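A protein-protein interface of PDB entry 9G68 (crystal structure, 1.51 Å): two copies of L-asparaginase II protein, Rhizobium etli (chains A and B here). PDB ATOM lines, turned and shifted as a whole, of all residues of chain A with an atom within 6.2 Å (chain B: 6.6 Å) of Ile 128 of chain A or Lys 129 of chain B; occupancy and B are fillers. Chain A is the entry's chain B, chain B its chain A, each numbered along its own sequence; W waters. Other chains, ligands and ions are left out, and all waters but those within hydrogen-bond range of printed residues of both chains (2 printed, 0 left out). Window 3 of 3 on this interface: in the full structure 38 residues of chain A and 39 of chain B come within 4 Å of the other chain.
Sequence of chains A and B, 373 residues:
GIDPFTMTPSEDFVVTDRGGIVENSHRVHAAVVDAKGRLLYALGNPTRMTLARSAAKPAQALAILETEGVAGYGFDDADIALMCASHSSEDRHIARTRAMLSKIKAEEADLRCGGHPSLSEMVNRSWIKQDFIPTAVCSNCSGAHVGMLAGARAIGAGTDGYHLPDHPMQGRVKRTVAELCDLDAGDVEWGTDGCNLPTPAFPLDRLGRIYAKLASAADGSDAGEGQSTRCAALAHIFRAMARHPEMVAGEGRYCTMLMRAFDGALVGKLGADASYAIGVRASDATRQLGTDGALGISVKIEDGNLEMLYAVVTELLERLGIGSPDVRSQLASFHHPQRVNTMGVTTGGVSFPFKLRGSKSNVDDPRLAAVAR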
ATOM      1  N   VAL A 123      24.734  -9.659 -31.702  1.00  0.00           N
ATOM      2  CA  VAL A 123      24.861  -8.736 -30.575  1.00  0.00           C
ATOM      3  C   VAL A 123      23.634  -7.840 -30.504  1.00  0.00           C
ATOM      4  O   VAL A 123      23.054  -7.621 -29.427  1.00  0.00           O
ATOM      5  CB  VAL A 123      26.161  -7.915 -30.688  1.00  0.00           C
ATOM      6  CG1 VAL A 123      26.218  -6.840 -29.606  1.00  0.00           C
ATOM      7  CG2 VAL A 123      27.394  -8.837 -30.638  1.00  0.00           C
ATOM      8  N   ASN A 124      23.192  -7.349 -31.659  1.00  0.00           N
ATOM      9  CA  ASN A 124      22.029  -6.488 -31.681  1.00  0.00           C
ATOM     10  C   ASN A 124      20.805  -7.202 -31.128  1.00  0.00           C
ATOM     11  O   ASN A 124      19.981  -6.588 -30.438  1.00  0.00           O
ATOM     12  CB  ASN A 124      21.773  -6.013 -33.096  1.00  0.00           C
ATOM     13  CG  ASN A 124      21.238  -4.632 -33.113  1.00  0.00           C
ATOM     14  OD1 ASN A 124      21.829  -3.735 -32.497  1.00  0.00           O
ATOM     15  ND2 ASN A 124      20.058  -4.450 -33.736  1.00  0.00           N
ATOM     16  N   ARG A 125      20.675  -8.500 -31.424  1.00  0.00           N
ATOM     17  CA  ARG A 125      19.585  -9.300 -30.872  1.00  0.00           C
ATOM     18  C   ARG A 125      19.610  -9.330 -29.345  1.00  0.00           C
ATOM     19  O   ARG A 125      18.561  -9.227 -28.694  1.00  0.00           O
ATOM     20  CB  ARG A 125      19.667 -10.715 -31.415  1.00  0.00           C
ATOM     21  CG  ARG A 125      18.703 -10.978 -32.466  1.00  0.00           C
ATOM     22  CD  ARG A 125      19.102 -10.383 -33.803  1.00  0.00           C
ATOM     23  NE  ARG A 125      18.171 -10.878 -34.816  1.00  0.00           N
ATOM     24  CZ  ARG A 125      18.033 -12.157 -35.144  1.00  0.00           C
ATOM     25  NH1 ARG A 125      18.831 -13.090 -34.642  1.00  0.00           N
ATOM     26  NH2 ARG A 125      17.065 -12.510 -35.988  1.00  0.00           N
ATOM     27  N   SER A 126      20.789  -9.539 -28.754  1.00  0.00           N
ATOM     28  CA  SER A 126      20.892  -9.497 -27.297  1.00  0.00           C
ATOM     29  C   SER A 126      20.498  -8.125 -26.759  1.00  0.00           C
ATOM     30  O   SER A 126      19.763  -8.019 -25.771  1.00  0.00           O
ATOM     31  CB  SER A 126      22.314  -9.854 -26.859  1.00  0.00           C
ATOM     32  OG  SER A 126      23.196  -8.757 -27.042  1.00  0.00           O
ATOM     33  N   TRP A 127      20.981  -7.055 -27.402  1.00  0.00           N
ATOM     34  CA  TRP A 127      20.630  -5.714 -26.949  1.00  0.00           C
ATOM     35  C   TRP A 127      19.124  -5.477 -27.019  1.00  0.00           C
ATOM     36  O   TRP A 127      18.540  -4.908 -26.086  1.00  0.00           O
ATOM     37  CB  TRP A 127      21.365  -4.671 -27.781  1.00  0.00           C
ATOM     38  CG  TRP A 127      22.857  -4.592 -27.569  1.00  0.00           C
ATOM     39  CD1 TRP A 127      23.624  -5.317 -26.694  1.00  0.00           C
ATOM     40  CD2 TRP A 127      23.751  -3.737 -28.274  1.00  0.00           C
ATOM     41  NE1 TRP A 127      24.955  -4.959 -26.819  1.00  0.00           N
ATOM     42  CE2 TRP A 127      25.058  -3.981 -27.772  1.00  0.00           C
ATOM     43  CE3 TRP A 127      23.577  -2.768 -29.272  1.00  0.00           C
ATOM     44  CZ2 TRP A 127      26.181  -3.302 -28.248  1.00  0.00           C
ATOM     45  CZ3 TRP A 127      24.696  -2.097 -29.745  1.00  0.00           C
ATOM     46  CH2 TRP A 127      25.981  -2.360 -29.224  1.00  0.00           C
ATOM     47  N   ILE A 128      18.475  -5.913 -28.112  1.00  0.00           N
ATOM     48  CA  ILE A 128      17.036  -5.689 -28.279  1.00  0.00           C
ATOM     49  C   ILE A 128      16.246  -6.329 -27.143  1.00  0.00           C
ATOM     50  O   ILE A 128      15.285  -5.740 -26.622  1.00  0.00           O
ATOM     51  CB  ILE A 128      16.554  -6.217 -29.647  1.00  0.00           C
ATOM     52  CG1 ILE A 128      17.051  -5.312 -30.782  1.00  0.00           C
ATOM     53  CG2 ILE A 128      15.019  -6.377 -29.658  1.00  0.00           C
ATOM     54  CD1 ILE A 128      17.045  -5.974 -32.169  1.00  0.00           C
ATOM     55  N   LYS A 129      16.626  -7.548 -26.749  1.00  0.00           N
ATOM     56  CA  LYS A 129      15.885  -8.232 -25.693  1.00  0.00           C
ATOM     57  C   LYS A 129      15.918  -7.459 -24.382  1.00  0.00           C
ATOM     58  O   LYS A 129      14.956  -7.531 -23.601  1.00  0.00           O
ATOM     59  CB  LYS A 129      16.433  -9.641 -25.473  1.00  0.00           C
ATOM     60  CG  LYS A 129      16.130 -10.592 -26.601  1.00  0.00           C
ATOM     61  CD  LYS A 129      16.592 -11.988 -26.261  1.00  0.00           C
ATOM     62  CE  LYS A 129      16.854 -12.796 -27.524  1.00  0.00           C
ATOM     63  NZ  LYS A 129      16.241 -14.145 -27.429  1.00  0.00           N
ATOM     64  N   GLN A 130      17.004  -6.736 -24.106  1.00  0.00           N
ATOM     65  CA  GLN A 130      17.133  -6.013 -22.848  1.00  0.00           C
ATOM     66  C   GLN A 130      16.723  -4.551 -22.968  1.00  0.00           C
ATOM     67  O   GLN A 130      16.830  -3.805 -21.988  1.00  0.00           O
ATOM     68  CB  GLN A 130      18.563  -6.125 -22.326  1.00  0.00           C
ATOM     69  CG  GLN A 130      19.040  -7.567 -22.232  1.00  0.00           C
ATOM     70  CD  GLN A 130      20.553  -7.687 -22.093  1.00  0.00           C
ATOM     71  OE1 GLN A 130      21.258  -6.689 -21.886  1.00  0.00           O
ATOM     72  NE2 GLN A 130      21.061  -8.919 -22.212  1.00  0.00           N
ATOM     73  N   ASP A 131      16.213  -4.136 -24.133  1.00  0.00           N
ATOM     74  CA  ASP A 131      15.949  -2.724 -24.427  1.00  0.00           C
ATOM     75  C   ASP A 131      17.190  -1.876 -24.134  1.00  0.00           C
ATOM     76  O   ASP A 131      17.084  -0.729 -23.700  1.00  0.00           O
ATOM     77  CB  ASP A 131      14.717  -2.206 -23.658  1.00  0.00           C
ATOM     78  CG  ASP A 131      13.397  -2.782 -24.193  1.00  0.00           C
ATOM     79  OD1 ASP A 131      12.973  -2.421 -25.328  1.00  0.00           O
ATOM     80  OD2 ASP A 131      12.788  -3.611 -23.480  1.00  0.00           O
ATOM     81  N   PHE A 132      18.376  -2.455 -24.370  1.00  0.00           N
ATOM     82  CA  PHE A 132      19.633  -1.760 -24.123  1.00  0.00           C
ATOM     83  C   PHE A 132      19.861  -0.682 -25.175  1.00  0.00           C
ATOM     84  O   PHE A 132      19.714  -0.922 -26.382  1.00  0.00           O
ATOM     85  CB  PHE A 132      20.808  -2.744 -24.111  1.00  0.00           C
ATOM     86  CG  PHE A 132      22.183  -2.082 -24.008  1.00  0.00           C
ATOM     87  CD1 PHE A 132      22.590  -1.441 -22.842  1.00  0.00           C
ATOM     88  CD2 PHE A 132      23.079  -2.136 -25.078  1.00  0.00           C
ATOM     89  CE1 PHE A 132      23.855  -0.851 -22.750  1.00  0.00           C
ATOM     90  CE2 PHE A 132      24.333  -1.546 -25.007  1.00  0.00           C
ATOM     91  CZ  PHE A 132      24.733  -0.905 -23.841  1.00  0.00           C
ATOM     92  N   ASN B 124      10.058  -6.326 -36.378  1.00  0.00           N
ATOM     93  CA  ASN B 124      11.032  -7.390 -36.192  1.00  0.00           C
ATOM     94  C   ASN B 124      11.719  -7.291 -34.840  1.00  0.00           C
ATOM     95  O   ASN B 124      11.994  -8.319 -34.211  1.00  0.00           O
ATOM     96  CB  ASN B 124      12.065  -7.369 -37.319  1.00  0.00           C
ATOM     97  CG  ASN B 124      12.708  -8.711 -37.515  1.00  0.00           C
ATOM     98  OD1 ASN B 124      12.010  -9.689 -37.769  1.00  0.00           O
ATOM     99  ND2 ASN B 124      14.051  -8.782 -37.375  1.00  0.00           N
ATOM    100  N   ARG B 125      12.010  -6.061 -34.371  1.00  0.00           N
ATOM    101  CA  ARG B 125      12.602  -5.893 -33.038  1.00  0.00           C
ATOM    102  C   ARG B 125      11.640  -6.366 -31.948  1.00  0.00           C
ATOM    103  O   ARG B 125      12.059  -6.971 -30.948  1.00  0.00           O
ATOM    104  CB  ARG B 125      12.995  -4.429 -32.797  1.00  0.00           C
ATOM    105  CG  ARG B 125      14.226  -3.967 -33.615  1.00  0.00           C
ATOM    106  CD  ARG B 125      14.758  -2.602 -33.141  1.00  0.00           C
ATOM    107  NE  ARG B 125      13.746  -1.547 -33.150  1.00  0.00           N
ATOM    108  CZ  ARG B 125      13.489  -0.760 -34.191  1.00  0.00           C
ATOM    109  NH1 ARG B 125      14.135  -0.901 -35.345  1.00  0.00           N
ATOM    110  NH2 ARG B 125      12.545   0.179 -34.081  1.00  0.00           N
ATOM    111  N   SER B 126      10.341  -6.097 -32.122  1.00  0.00           N
ATOM    112  CA  SER B 126       9.352  -6.608 -31.178  1.00  0.00           C
ATOM    113  C   SER B 126       9.343  -8.140 -31.169  1.00  0.00           C
ATOM    114  O   SER B 126       9.274  -8.770 -30.105  1.00  0.00           O
ATOM    115  CB  SER B 126       7.977  -6.033 -31.539  1.00  0.00           C
ATOM    116  OG  SER B 126       6.994  -6.393 -30.580  1.00  0.00           O
ATOM    117  N   TRP B 127       9.425  -8.752 -32.347  1.00  0.00           N
ATOM    118  CA  TRP B 127       9.518 -10.207 -32.446  1.00  0.00           C
ATOM    119  C   TRP B 127      10.762 -10.734 -31.742  1.00  0.00           C
ATOM    120  O   TRP B 127      10.694 -11.717 -31.005  1.00  0.00           O
ATOM    121  CB  TRP B 127       9.561 -10.609 -33.919  1.00  0.00           C
ATOM    122  CG  TRP B 127       8.275 -10.498 -34.624  1.00  0.00           C
ATOM    123  CD1 TRP B 127       7.061 -10.060 -34.112  1.00  0.00           C
ATOM    124  CD2 TRP B 127       8.044 -10.850 -35.979  1.00  0.00           C
ATOM    125  NE1 TRP B 127       6.090 -10.121 -35.103  1.00  0.00           N
ATOM    126  CE2 TRP B 127       6.674 -10.602 -36.254  1.00  0.00           C
ATOM    127  CE3 TRP B 127       8.874 -11.328 -37.013  1.00  0.00           C
ATOM    128  CZ2 TRP B 127       6.123 -10.834 -37.507  1.00  0.00           C
ATOM    129  CZ3 TRP B 127       8.303 -11.580 -38.254  1.00  0.00           C
ATOM    130  CH2 TRP B 127       6.951 -11.338 -38.481  1.00  0.00           C
ATOM    131  N   ILE B 128      11.924 -10.110 -31.991  1.00  0.00           N
ATOM    132  CA  ILE B 128      13.170 -10.585 -31.384  1.00  0.00           C
ATOM    133  C   ILE B 128      13.081 -10.506 -29.873  1.00  0.00           C
ATOM    134  O   ILE B 128      13.479 -11.437 -29.157  1.00  0.00           O
ATOM    135  CB  ILE B 128      14.369  -9.768 -31.903  1.00  0.00           C
ATOM    136  CG1 ILE B 128      14.695 -10.154 -33.356  1.00  0.00           C
ATOM    137  CG2 ILE B 128      15.560  -9.922 -30.960  1.00  0.00           C
ATOM    138  CD1 ILE B 128      15.520  -9.097 -34.051  1.00  0.00           C
ATOM    139  N   LYS B 129      12.548  -9.394 -29.369  1.00  0.00           N
ATOM    140  CA  LYS B 129      12.368  -9.228 -27.934  1.00  0.00           C
ATOM    141  C   LYS B 129      11.572 -10.383 -27.335  1.00  0.00           C
ATOM    142  O   LYS B 129      11.824 -10.783 -26.189  1.00  0.00           O
ATOM    143  CB  LYS B 129      11.661  -7.894 -27.651  1.00  0.00           C
ATOM    144  CG  LYS B 129      11.462  -7.643 -26.184  1.00  0.00           C
ATOM    145  CD  LYS B 129      10.822  -6.279 -25.885  1.00  0.00           C
ATOM    146  CE  LYS B 129      10.576  -6.142 -24.355  1.00  0.00           C
ATOM    147  NZ  LYS B 129      10.131  -4.769 -23.934  1.00  0.00           N
ATOM    148  N   GLN B 130      10.607 -10.925 -28.081  1.00  0.00           N
ATOM    149  CA  GLN B 130       9.687 -11.919 -27.527  1.00  0.00           C
ATOM    150  C   GLN B 130      10.012 -13.334 -27.975  1.00  0.00           C
ATOM    151  O   GLN B 130       9.180 -14.233 -27.805  1.00  0.00           O
ATOM    152  CB  GLN B 130       8.247 -11.541 -27.887  1.00  0.00           C
ATOM    153  CG  GLN B 130       7.876 -10.160 -27.328  1.00  0.00           C
ATOM    154  CD  GLN B 130       6.549  -9.622 -27.867  1.00  0.00           C
ATOM    155  OE1 GLN B 130       5.474  -9.935 -27.334  1.00  0.00           O
ATOM    156  NE2 GLN B 130       6.618  -8.802 -28.913  1.00  0.00           N
ATOM    157  N   ASP B 131      11.201 -13.542 -28.552  1.00  0.00           N
ATOM    158  CA  ASP B 131      11.621 -14.850 -29.069  1.00  0.00           C
ATOM    159  C   ASP B 131      10.609 -15.439 -30.054  1.00  0.00           C
ATOM    160  O   ASP B 131      10.385 -16.657 -30.101  1.00  0.00           O
ATOM    161  CB  ASP B 131      11.876 -15.830 -27.926  1.00  0.00           C
ATOM    162  CG  ASP B 131      13.026 -15.405 -27.027  1.00  0.00           C
ATOM    163  OD1 ASP B 131      14.072 -14.980 -27.560  1.00  0.00           O
ATOM    164  OD2 ASP B 131      12.888 -15.517 -25.785  1.00  0.00           O
ATOM    165  N   PHE B 132       9.988 -14.585 -30.857  1.00  0.00           N
ATOM    166  CA  PHE B 132       8.933 -15.035 -31.752  1.00  0.00           C
ATOM    167  C   PHE B 132       9.517 -15.549 -33.062  1.00  0.00           C
ATOM    168  O   PHE B 132      10.300 -14.851 -33.713  1.00  0.00           O
ATOM    169  CB  PHE B 132       7.949 -13.916 -32.050  1.00  0.00           C
ATOM    170  CG  PHE B 132       6.863 -14.333 -33.012  1.00  0.00           C
ATOM    171  CD1 PHE B 132       5.872 -15.238 -32.625  1.00  0.00           C
ATOM    172  CD2 PHE B 132       6.842 -13.842 -34.320  1.00  0.00           C
ATOM    173  CE1 PHE B 132       4.876 -15.636 -33.523  1.00  0.00           C
ATOM    174  CE2 PHE B 132       5.844 -14.234 -35.219  1.00  0.00           C
ATOM    175  CZ  PHE B 132       4.872 -15.124 -34.831  1.00  0.00           C
HETATM  176  O   HOH W   1      14.984 -13.679 -29.911  1.00  0.00           O
HETATM  177  O   HOH W   2      15.513 -11.410 -37.526  1.00  0.00           O
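The side-chain amino group (NZ) of Lys 129 of chain B is in salt-bridge range of the side-chain carboxylate (OD2) of Asp 131 of chain A (2.9 Å). OD2 of Asp 131 of chain B is in salt-bridge range of NZ of Lys 129 of chain A (3.98 Å).
Among the printed residues, merely in contact across the chains: Arg 125 of chain A with Ile 128 of chain B (3.3 Å), Ile 128 of chain A with Arg 125 of chain B (3.3 Å), Ile 128 of chain A with Ile 128 of chain B (3.8 Å), Ile 128 of chain A with Lys 129 of chain B (3.9 Å) and Lys 129 of chain A with Ile 128 of chain B (3.8 Å).
Of chain B, only Arg 125 (3.3 Å), Ile 128 (3.8 Å) and Lys 129 (3.9 Å) come within 4 Å of Ile 128 of chain A. Of chain A, only Ile 128 and Asp 131 come within 4 Å of Lys 129 of chain B. Of the printed residues of chain A, Arg 125 of chain B touches Ile 128 (3.3 Å). Printed residues of chain A within 4 Å of Ile 128 of chain B: Arg 125 (3.3 Å), Ile 128 (3.8 Å) and Lys 129 (3.8 Å). Of the printed residues of chain B, Asp 131 of chain A touches Lys 129. Of the printed residues of chain B, Lys 129 of chain A touches Ile 128 (3.8 Å) and Asp 131 (2.3 Å). Ser 126 of chain B touches none of the printed residues of chain A. The nearest printed residue of chain B that does not touch Lys 129 of chain A is Lys 129 of chain B (4.2 Å).
Hydrophobic or aromatic side chains of chain B within 4 Å of the printed part of chain A: Ile 128. Hydrophobic or aromatic side chains of chain A within 4 Å of the printed part of chain B: Ile 128. Among the printed residues, 7 pairs touch across the chains. Among the printed residues, Asp or Glu carboxylates within 4 Å of a Lys or Arg side-chain nitrogen of the other chain: Lys 129 of chain A with Asp 131 of chain B and Asp 131 of chain A with Lys 129 of chain B.
Arg 125 of chain A touches Ile 128 of chain B, and with the chains exchanged Ile 128 of chain A touches Arg 125 of chain B. Ile 128 of chain B touches its own counterpart, Ile 128 of chain A. Ile 128 of chain A touches Lys 129 of chain B, and with the chains exchanged Lys 129 of chain A touches Ile 128 of chain B. Lys 129 of chain A touches Asp 131 of chain B, and with the chains exchanged Asp 131 of chain A touches Lys 129 of chain B. 9 positions are printed for both chains. Of the 7 pairs that touch across the chains among the printed residues, 7 have their exchanged pair printed and touching as well.
Water W2 lies within hydrogen-bond range of the guanidinium group of Arg 125 of chain A (2.4 Å) and the side-chain amide nitrogen of Asn 124 of chain B (3.0 Å). Water W1 lies within hydrogen-bond range of the backbone carbonyl oxygen (O) of Ile 128 of chain B (2.8 Å), the side-chain amino group (NZ) of Lys 129 of chain A (2.8 Å) and the side-chain carboxylate (OD1) of Asp 131 of chain B (2.8 Å).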
